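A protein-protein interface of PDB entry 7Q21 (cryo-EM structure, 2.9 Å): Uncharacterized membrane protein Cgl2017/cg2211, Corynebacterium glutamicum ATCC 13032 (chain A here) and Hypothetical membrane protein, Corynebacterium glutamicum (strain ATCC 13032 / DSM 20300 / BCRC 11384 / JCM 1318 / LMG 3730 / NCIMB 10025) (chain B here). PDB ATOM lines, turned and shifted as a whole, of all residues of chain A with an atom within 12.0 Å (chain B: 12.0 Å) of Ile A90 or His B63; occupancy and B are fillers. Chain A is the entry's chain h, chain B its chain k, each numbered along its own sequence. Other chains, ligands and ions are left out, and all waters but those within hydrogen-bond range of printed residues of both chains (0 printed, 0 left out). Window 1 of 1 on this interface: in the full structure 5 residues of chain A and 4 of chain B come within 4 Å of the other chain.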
ATOM      1  N   GLN A  86     -14.330  15.348  17.419  1.00  0.00           N
ATOM      2  CA  GLN A  86     -13.911  14.985  16.074  1.00  0.00           C
ATOM      3  C   GLN A  86     -14.442  13.595  15.732  1.00  0.00           C
ATOM      4  O   GLN A  86     -14.439  12.704  16.580  1.00  0.00           O
ATOM      5  CB  GLN A  86     -12.381  15.031  16.012  1.00  0.00           C
ATOM      6  CG  GLN A  86     -11.792  14.793  14.624  1.00  0.00           C
ATOM      7  CD  GLN A  86     -12.113  15.898  13.647  1.00  0.00           C
ATOM      8  OE1 GLN A  86     -11.859  17.076  13.895  1.00  0.00           O
ATOM      9  NE2 GLN A  86     -12.672  15.521  12.509  1.00  0.00           N
ATOM     10  N   VAL A  87     -14.914  13.431  14.491  1.00  0.00           N
ATOM     11  CA  VAL A  87     -15.573  12.217  14.038  1.00  0.00           C
ATOM     12  C   VAL A  87     -14.589  11.047  14.039  1.00  0.00           C
ATOM     13  O   VAL A  87     -14.911   9.981  14.560  1.00  0.00           O
ATOM     14  CB  VAL A  87     -16.257  12.447  12.673  1.00  0.00           C
ATOM     15  CG1 VAL A  87     -16.673  11.162  11.966  1.00  0.00           C
ATOM     16  CG2 VAL A  87     -17.451  13.382  12.797  1.00  0.00           C
ATOM     17  N   ARG A  88     -13.400  11.274  13.464  1.00  0.00           N
ATOM     18  CA  ARG A  88     -12.313  10.305  13.435  1.00  0.00           C
ATOM     19  C   ARG A  88     -12.769   9.022  12.737  1.00  0.00           C
ATOM     20  O   ARG A  88     -12.967   7.992  13.372  1.00  0.00           O
ATOM     21  CB  ARG A  88     -11.756  10.083  14.848  1.00  0.00           C
ATOM     22  CG  ARG A  88     -10.441   9.315  14.898  1.00  0.00           C
ATOM     23  CD  ARG A  88      -9.856   9.214  16.300  1.00  0.00           C
ATOM     24  NE  ARG A  88      -9.096  10.380  16.747  1.00  0.00           N
ATOM     25  CZ  ARG A  88      -9.600  11.440  17.380  1.00  0.00           C
ATOM     26  NH1 ARG A  88      -8.801  12.432  17.732  1.00  0.00           N
ATOM     27  NH2 ARG A  88     -10.890  11.511  17.659  1.00  0.00           N
ATOM     28  N   THR A  89     -13.045   9.135  11.433  1.00  0.00           N
ATOM     29  CA  THR A  89     -13.372   7.995  10.590  1.00  0.00           C
ATOM     30  C   THR A  89     -12.474   8.019   9.357  1.00  0.00           C
ATOM     31  O   THR A  89     -11.637   8.910   9.220  1.00  0.00           O
ATOM     32  CB  THR A  89     -14.861   7.963  10.206  1.00  0.00           C
ATOM     33  OG1 THR A  89     -15.216   9.247   9.688  1.00  0.00           O
ATOM     34  CG2 THR A  89     -15.761   7.582  11.363  1.00  0.00           C
ATOM     35  N   ILE A  90     -12.667   7.038   8.465  1.00  0.00           N
ATOM     36  CA  ILE A  90     -11.943   6.952   7.208  1.00  0.00           C
ATOM     37  C   ILE A  90     -12.958   6.659   6.111  1.00  0.00           C
ATOM     38  O   ILE A  90     -13.687   5.675   6.186  1.00  0.00           O
ATOM     39  CB  ILE A  90     -10.844   5.866   7.256  1.00  0.00           C
ATOM     40  CG1 ILE A  90      -9.819   6.064   8.382  1.00  0.00           C
ATOM     41  CG2 ILE A  90     -10.193   5.692   5.884  1.00  0.00           C
ATOM     42  CD1 ILE A  90      -8.815   7.181   8.177  1.00  0.00           C
ATOM     43  N   THR A  91     -12.980   7.527   5.093  1.00  0.00           N
ATOM     44  CA  THR A  91     -13.829   7.328   3.931  1.00  0.00           C
ATOM     45  C   THR A  91     -12.968   6.842   2.767  1.00  0.00           C
ATOM     46  O   THR A  91     -11.757   7.068   2.751  1.00  0.00           O
ATOM     47  CB  THR A  91     -14.646   8.588   3.619  1.00  0.00           C
ATOM     48  OG1 THR A  91     -15.225   9.077   4.831  1.00  0.00           O
ATOM     49  CG2 THR A  91     -15.746   8.338   2.611  1.00  0.00           C
ATOM     50  N   SER A  92     -13.612   6.171   1.806  1.00  0.00           N
ATOM     51  CA  SER A  92     -13.005   5.576   0.624  1.00  0.00           C
ATOM     52  C   SER A  92     -11.964   6.503  -0.001  1.00  0.00           C
ATOM     53  O   SER A  92     -12.283   7.629  -0.369  1.00  0.00           O
ATOM     54  CB  SER A  92     -14.077   5.215  -0.377  1.00  0.00           C
ATOM     55  OG  SER A  92     -14.590   6.376  -1.027  1.00  0.00           O
ATOM     56  N   ARG A  93     -10.721   6.012  -0.104  1.00  0.00           N
ATOM     57  CA  ARG A  93      -9.588   6.712  -0.691  1.00  0.00           C
ATOM     58  C   ARG A  93      -9.356   8.072  -0.026  1.00  0.00           C
ATOM     59  O   ARG A  93      -9.092   9.051  -0.710  1.00  0.00           O
ATOM     60  CB  ARG A  93      -9.717   6.794  -2.215  1.00  0.00           C
ATOM     61  CG  ARG A  93      -9.445   5.479  -2.931  1.00  0.00           C
ATOM     62  CD  ARG A  93     -10.614   4.517  -2.978  1.00  0.00           C
ATOM     63  NE  ARG A  93     -11.782   5.064  -3.662  1.00  0.00           N
ATOM     64  CZ  ARG A  93     -12.992   4.508  -3.679  1.00  0.00           C
ATOM     65  NH1 ARG A  93     -13.216   3.361  -3.057  1.00  0.00           N
ATOM     66  NH2 ARG A  93     -13.981   5.108  -4.318  1.00  0.00           N
ATOM     67  N   ASN A  94      -9.514   8.122   1.300  1.00  0.00           N
ATOM     68  CA  ASN A  94      -9.168   9.270   2.116  1.00  0.00           C
ATOM     69  C   ASN A  94      -8.148   8.803   3.149  1.00  0.00           C
ATOM     70  O   ASN A  94      -8.294   7.737   3.752  1.00  0.00           O
ATOM     71  CB  ASN A  94     -10.396   9.897   2.792  1.00  0.00           C
ATOM     72  CG  ASN A  94     -10.079  11.173   3.544  1.00  0.00           C
ATOM     73  OD1 ASN A  94      -9.572  12.135   2.971  1.00  0.00           O
ATOM     74  ND2 ASN A  94     -10.369  11.185   4.833  1.00  0.00           N
ATOM     75  N   LYS A  95      -7.131   9.637   3.384  1.00  0.00           N
ATOM     76  CA  LYS A  95      -6.007   9.227   4.205  1.00  0.00           C
ATOM     77  C   LYS A  95      -6.193   9.736   5.639  1.00  0.00           C
ATOM     78  O   LYS A  95      -6.785  10.794   5.848  1.00  0.00           O
ATOM     79  CB  LYS A  95      -4.692   9.670   3.552  1.00  0.00           C
ATOM     80  CG  LYS A  95      -4.066   8.673   2.579  1.00  0.00           C
ATOM     81  CD  LYS A  95      -4.742   8.623   1.232  1.00  0.00           C
ATOM     82  CE  LYS A  95      -4.208   7.523   0.336  1.00  0.00           C
ATOM     83  NZ  LYS A  95      -4.984   7.413  -0.920  1.00  0.00           N
ATOM     84  N   PRO A  96      -5.719   8.984   6.664  1.00  0.00           N
ATOM     85  CA  PRO A  96      -5.855   9.406   8.060  1.00  0.00           C
ATOM     86  C   PRO A  96      -5.026  10.647   8.375  1.00  0.00           C
ATOM     87  O   PRO A  96      -4.139  11.020   7.610  1.00  0.00           O
ATOM     88  CB  PRO A  96      -5.347   8.189   8.853  1.00  0.00           C
ATOM     89  CG  PRO A  96      -4.392   7.514   7.905  1.00  0.00           C
ATOM     90  CD  PRO A  96      -5.037   7.682   6.544  1.00  0.00           C
ATOM     91  N   VAL A  97      -5.297  11.235   9.545  1.00  0.00           N
ATOM     92  CA  VAL A  97      -4.573  12.398  10.036  1.00  0.00           C
ATOM     93  C   VAL A  97      -3.108  12.010  10.209  1.00  0.00           C
ATOM     94  O   VAL A  97      -2.800  10.977  10.802  1.00  0.00           O
ATOM     95  CB  VAL A  97      -5.183  12.947  11.344  1.00  0.00           C
ATOM     96  CG1 VAL A  97      -4.417  14.154  11.869  1.00  0.00           C
ATOM     97  CG2 VAL A  97      -6.660  13.281  11.192  1.00  0.00           C
ATOM     98  N   GLY A  98      -2.221  12.843   9.648  1.00  0.00           N
ATOM     99  CA  GLY A  98      -0.786  12.609   9.679  1.00  0.00           C
ATOM    100  C   GLY A  98      -0.281  11.966   8.389  1.00  0.00           C
ATOM    101  O   GLY A  98       0.585  11.093   8.431  1.00  0.00           O
ATOM    102  N   HIS A  99      -0.859  12.398   7.264  1.00  0.00           N
ATOM    103  CA  HIS A  99      -0.424  11.990   5.939  1.00  0.00           C
ATOM    104  C   HIS A  99       0.083  13.213   5.186  1.00  0.00           C
ATOM    105  O   HIS A  99      -0.546  14.269   5.224  1.00  0.00           O
ATOM    106  CB  HIS A  99      -1.535  11.229   5.192  1.00  0.00           C
ATOM    107  CG  HIS A  99      -1.374  11.194   3.708  1.00  0.00           C
ATOM    108  ND1 HIS A  99      -0.487  10.346   3.069  1.00  0.00           N
ATOM    109  CD2 HIS A  99      -1.983  11.906   2.737  1.00  0.00           C
ATOM    110  CE1 HIS A  99      -0.574  10.527   1.767  1.00  0.00           C
ATOM    111  NE2 HIS A  99      -1.494  11.469   1.536  1.00  0.00           N
ATOM    112  N   ASP B  56     -27.023   0.211   5.690  1.00  0.00           N
ATOM    113  CA  ASP B  56     -25.732   0.884   5.762  1.00  0.00           C
ATOM    114  C   ASP B  56     -24.678  -0.030   6.383  1.00  0.00           C
ATOM    115  O   ASP B  56     -23.521  -0.007   5.969  1.00  0.00           O
ATOM    116  CB  ASP B  56     -25.810   2.230   6.491  1.00  0.00           C
ATOM    117  CG  ASP B  56     -24.447   2.769   6.902  1.00  0.00           C
ATOM    118  OD1 ASP B  56     -23.585   2.934   6.012  1.00  0.00           O
ATOM    119  OD2 ASP B  56     -24.244   2.979   8.111  1.00  0.00           O
ATOM    120  N   VAL B  57     -25.086  -0.819   7.383  1.00  0.00           N
ATOM    121  CA  VAL B  57     -24.191  -1.739   8.069  1.00  0.00           C
ATOM    122  C   VAL B  57     -23.985  -2.986   7.209  1.00  0.00           C
ATOM    123  O   VAL B  57     -23.279  -3.910   7.611  1.00  0.00           O
ATOM    124  CB  VAL B  57     -24.700  -2.099   9.479  1.00  0.00           C
ATOM    125  CG1 VAL B  57     -24.772  -0.883  10.389  1.00  0.00           C
ATOM    126  CG2 VAL B  57     -26.034  -2.823   9.438  1.00  0.00           C
ATOM    127  N   ASN B  58     -24.627  -3.001   6.035  1.00  0.00           N
ATOM    128  CA  ASN B  58     -24.489  -4.080   5.073  1.00  0.00           C
ATOM    129  C   ASN B  58     -23.404  -3.740   4.051  1.00  0.00           C
ATOM    130  O   ASN B  58     -22.628  -4.614   3.669  1.00  0.00           O
ATOM    131  CB  ASN B  58     -25.821  -4.424   4.402  1.00  0.00           C
ATOM    132  CG  ASN B  58     -25.676  -5.470   3.317  1.00  0.00           C
ATOM    133  OD1 ASN B  58     -25.532  -5.135   2.143  1.00  0.00           O
ATOM    134  ND2 ASN B  58     -25.679  -6.736   3.700  1.00  0.00           N
ATOM    135  N   SER B  59     -23.390  -2.481   3.591  1.00  0.00           N
ATOM    136  CA  SER B  59     -22.395  -2.002   2.645  1.00  0.00           C
ATOM    137  C   SER B  59     -21.801  -0.683   3.141  1.00  0.00           C
ATOM    138  O   SER B  59     -22.048   0.369   2.551  1.00  0.00           O
ATOM    139  CB  SER B  59     -22.977  -1.880   1.256  1.00  0.00           C
ATOM    140  OG  SER B  59     -23.960  -0.858   1.205  1.00  0.00           O
ATOM    141  N   PRO B  60     -20.992  -0.692   4.229  1.00  0.00           N
ATOM    142  CA  PRO B  60     -20.486   0.550   4.815  1.00  0.00           C
ATOM    143  C   PRO B  60     -19.437   1.191   3.912  1.00  0.00           C
ATOM    144  O   PRO B  60     -18.746   0.495   3.170  1.00  0.00           O
ATOM    145  CB  PRO B  60     -19.869   0.094   6.145  1.00  0.00           C
ATOM    146  CG  PRO B  60     -19.447  -1.337   5.888  1.00  0.00           C
ATOM    147  CD  PRO B  60     -20.479  -1.887   4.925  1.00  0.00           C
ATOM    148  N   THR B  61     -19.355   2.525   3.976  1.00  0.00           N
ATOM    149  CA  THR B  61     -18.397   3.296   3.196  1.00  0.00           C
ATOM    150  C   THR B  61     -17.431   4.052   4.109  1.00  0.00           C
ATOM    151  O   THR B  61     -16.451   4.621   3.628  1.00  0.00           O
ATOM    152  CB  THR B  61     -19.098   4.231   2.202  1.00  0.00           C
ATOM    153  OG1 THR B  61     -20.142   4.923   2.888  1.00  0.00           O
ATOM    154  CG2 THR B  61     -19.658   3.505   0.998  1.00  0.00           C
ATOM    155  N   SER B  62     -17.717   4.055   5.418  1.00  0.00           N
ATOM    156  CA  SER B  62     -16.872   4.704   6.409  1.00  0.00           C
ATOM    157  C   SER B  62     -16.480   3.711   7.500  1.00  0.00           C
ATOM    158  O   SER B  62     -17.328   2.984   8.016  1.00  0.00           O
ATOM    159  CB  SER B  62     -17.543   5.926   6.979  1.00  0.00           C
ATOM    160  OG  SER B  62     -18.828   5.605   7.486  1.00  0.00           O
ATOM    161  N   HIS B  63     -15.182   3.691   7.826  1.00  0.00           N
ATOM    162  CA  HIS B  63     -14.627   2.805   8.838  1.00  0.00           C
ATOM    163  C   HIS B  63     -14.289   3.602  10.093  1.00  0.00           C
ATOM    164  O   HIS B  63     -13.878   4.758  10.003  1.00  0.00           O
ATOM    165  CB  HIS B  63     -13.393   2.058   8.302  1.00  0.00           C
ATOM    166  CG  HIS B  63     -13.644   1.223   7.090  1.00  0.00           C
ATOM    167  ND1 HIS B  63     -14.894   0.721   6.780  1.00  0.00           N
ATOM    168  CD2 HIS B  63     -12.809   0.783   6.122  1.00  0.00           C
ATOM    169  CE1 HIS B  63     -14.821   0.019   5.667  1.00  0.00           C
ATOM    170  NE2 HIS B  63     -13.551   0.041   5.244  1.00  0.00           N
ATOM    171  N   LYS B  64     -14.449   2.955  11.254  1.00  0.00           N
ATOM    172  CA  LYS B  64     -14.104   3.536  12.541  1.00  0.00           C
ATOM    173  C   LYS B  64     -12.583   3.596  12.667  1.00  0.00           C
ATOM    174  O   LYS B  64     -11.961   2.680  13.205  1.00  0.00           O
ATOM    175  CB  LYS B  64     -14.764   2.747  13.678  1.00  0.00           C
ATOM    176  CG  LYS B  64     -16.290   2.716  13.671  1.00  0.00           C
ATOM    177  CD  LYS B  64     -16.962   4.072  13.817  1.00  0.00           C
ATOM    178  CE  LYS B  64     -16.745   4.721  15.168  1.00  0.00           C
ATOM    179  NZ  LYS B  64     -17.476   6.006  15.284  1.00  0.00           N
ATOM    180  N   ILE B  65     -12.013   4.695  12.148  1.00  0.00           N
ATOM    181  CA  ILE B  65     -10.582   4.972  12.096  1.00  0.00           C
ATOM    182  C   ILE B  65      -9.789   3.695  11.780  1.00  0.00           C
ATOM    183  O   ILE B  65      -8.729   3.828  11.145  1.00  0.00           O
ATOM    184  CB  ILE B  65     -10.072   5.718  13.355  1.00  0.00           C
ATOM    185  CG1 ILE B  65      -8.749   6.451  13.104  1.00  0.00           C
ATOM    186  CG2 ILE B  65      -9.974   4.810  14.575  1.00  0.00           C
ATOM    187  CD1 ILE B  65      -8.781   7.444  11.963  1.00  0.00           C
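The backbone carbonyl oxygen (O) of Ile A90 lies within hydrogen-bond range of the backbone NH (N) of His B63 (3.0 Å).
O of Arg A88 touches N of Ile B65, 3.6 Å away. Thr A89 touches His B63. Thr A89 touches Ile B65 (CA to N, 3.9 Å). Ile A90 touches Thr B61. Ile A90 touches Ser B62 (O to CA, 3.3 Å). CG1 of Ile A90 touches O of Ile B65, at 3.7 Å. O of Thr B61 touches CA of Thr A91 (3.8 Å). Thr B61 touches Ser A92 (O to N, 3.7 Å).
His B63 touches just these residues of chain A: Thr A89 (3.3 Å) and Ile A90 (3.0 Å). Of the printed residues of chain B, Thr A89 touches His B63 (3.3 Å) and Ile B65 (3.9 Å). Thr A91 touches just one residue of chain B: Thr B61 (3.8 Å). Ser A92 touches one residue of chain B. No residue of chain A comes within 4 Å of Pro B60. Ser B62 touches one residue of chain A. No residue of chain A comes within 4 Å of Lys B64. Of the printed residues of chain B, Arg A88 touches Ile B65 (3.6 Å). The nearest residue of chain A that does not touch His B63 is Arg A88 (4.8 Å).
Of the 10 printed residues of chain B, 4 touch a printed residue of chain A. Hydrophobic or aromatic side chains of chain B within 4 Å of the printed part of chain A: Ile B65. Printed residues of chain A that touch a printed residue of chain B: Arg A88, Thr A89, Ile A90, Thr A91 and Ser A92. Among the printed residues, 9 pairs touch across the chains. Among the printed residues, no Asp or Glu carboxylate lies within 4 Å of a Lys or Arg side-chain nitrogen of the other chain.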
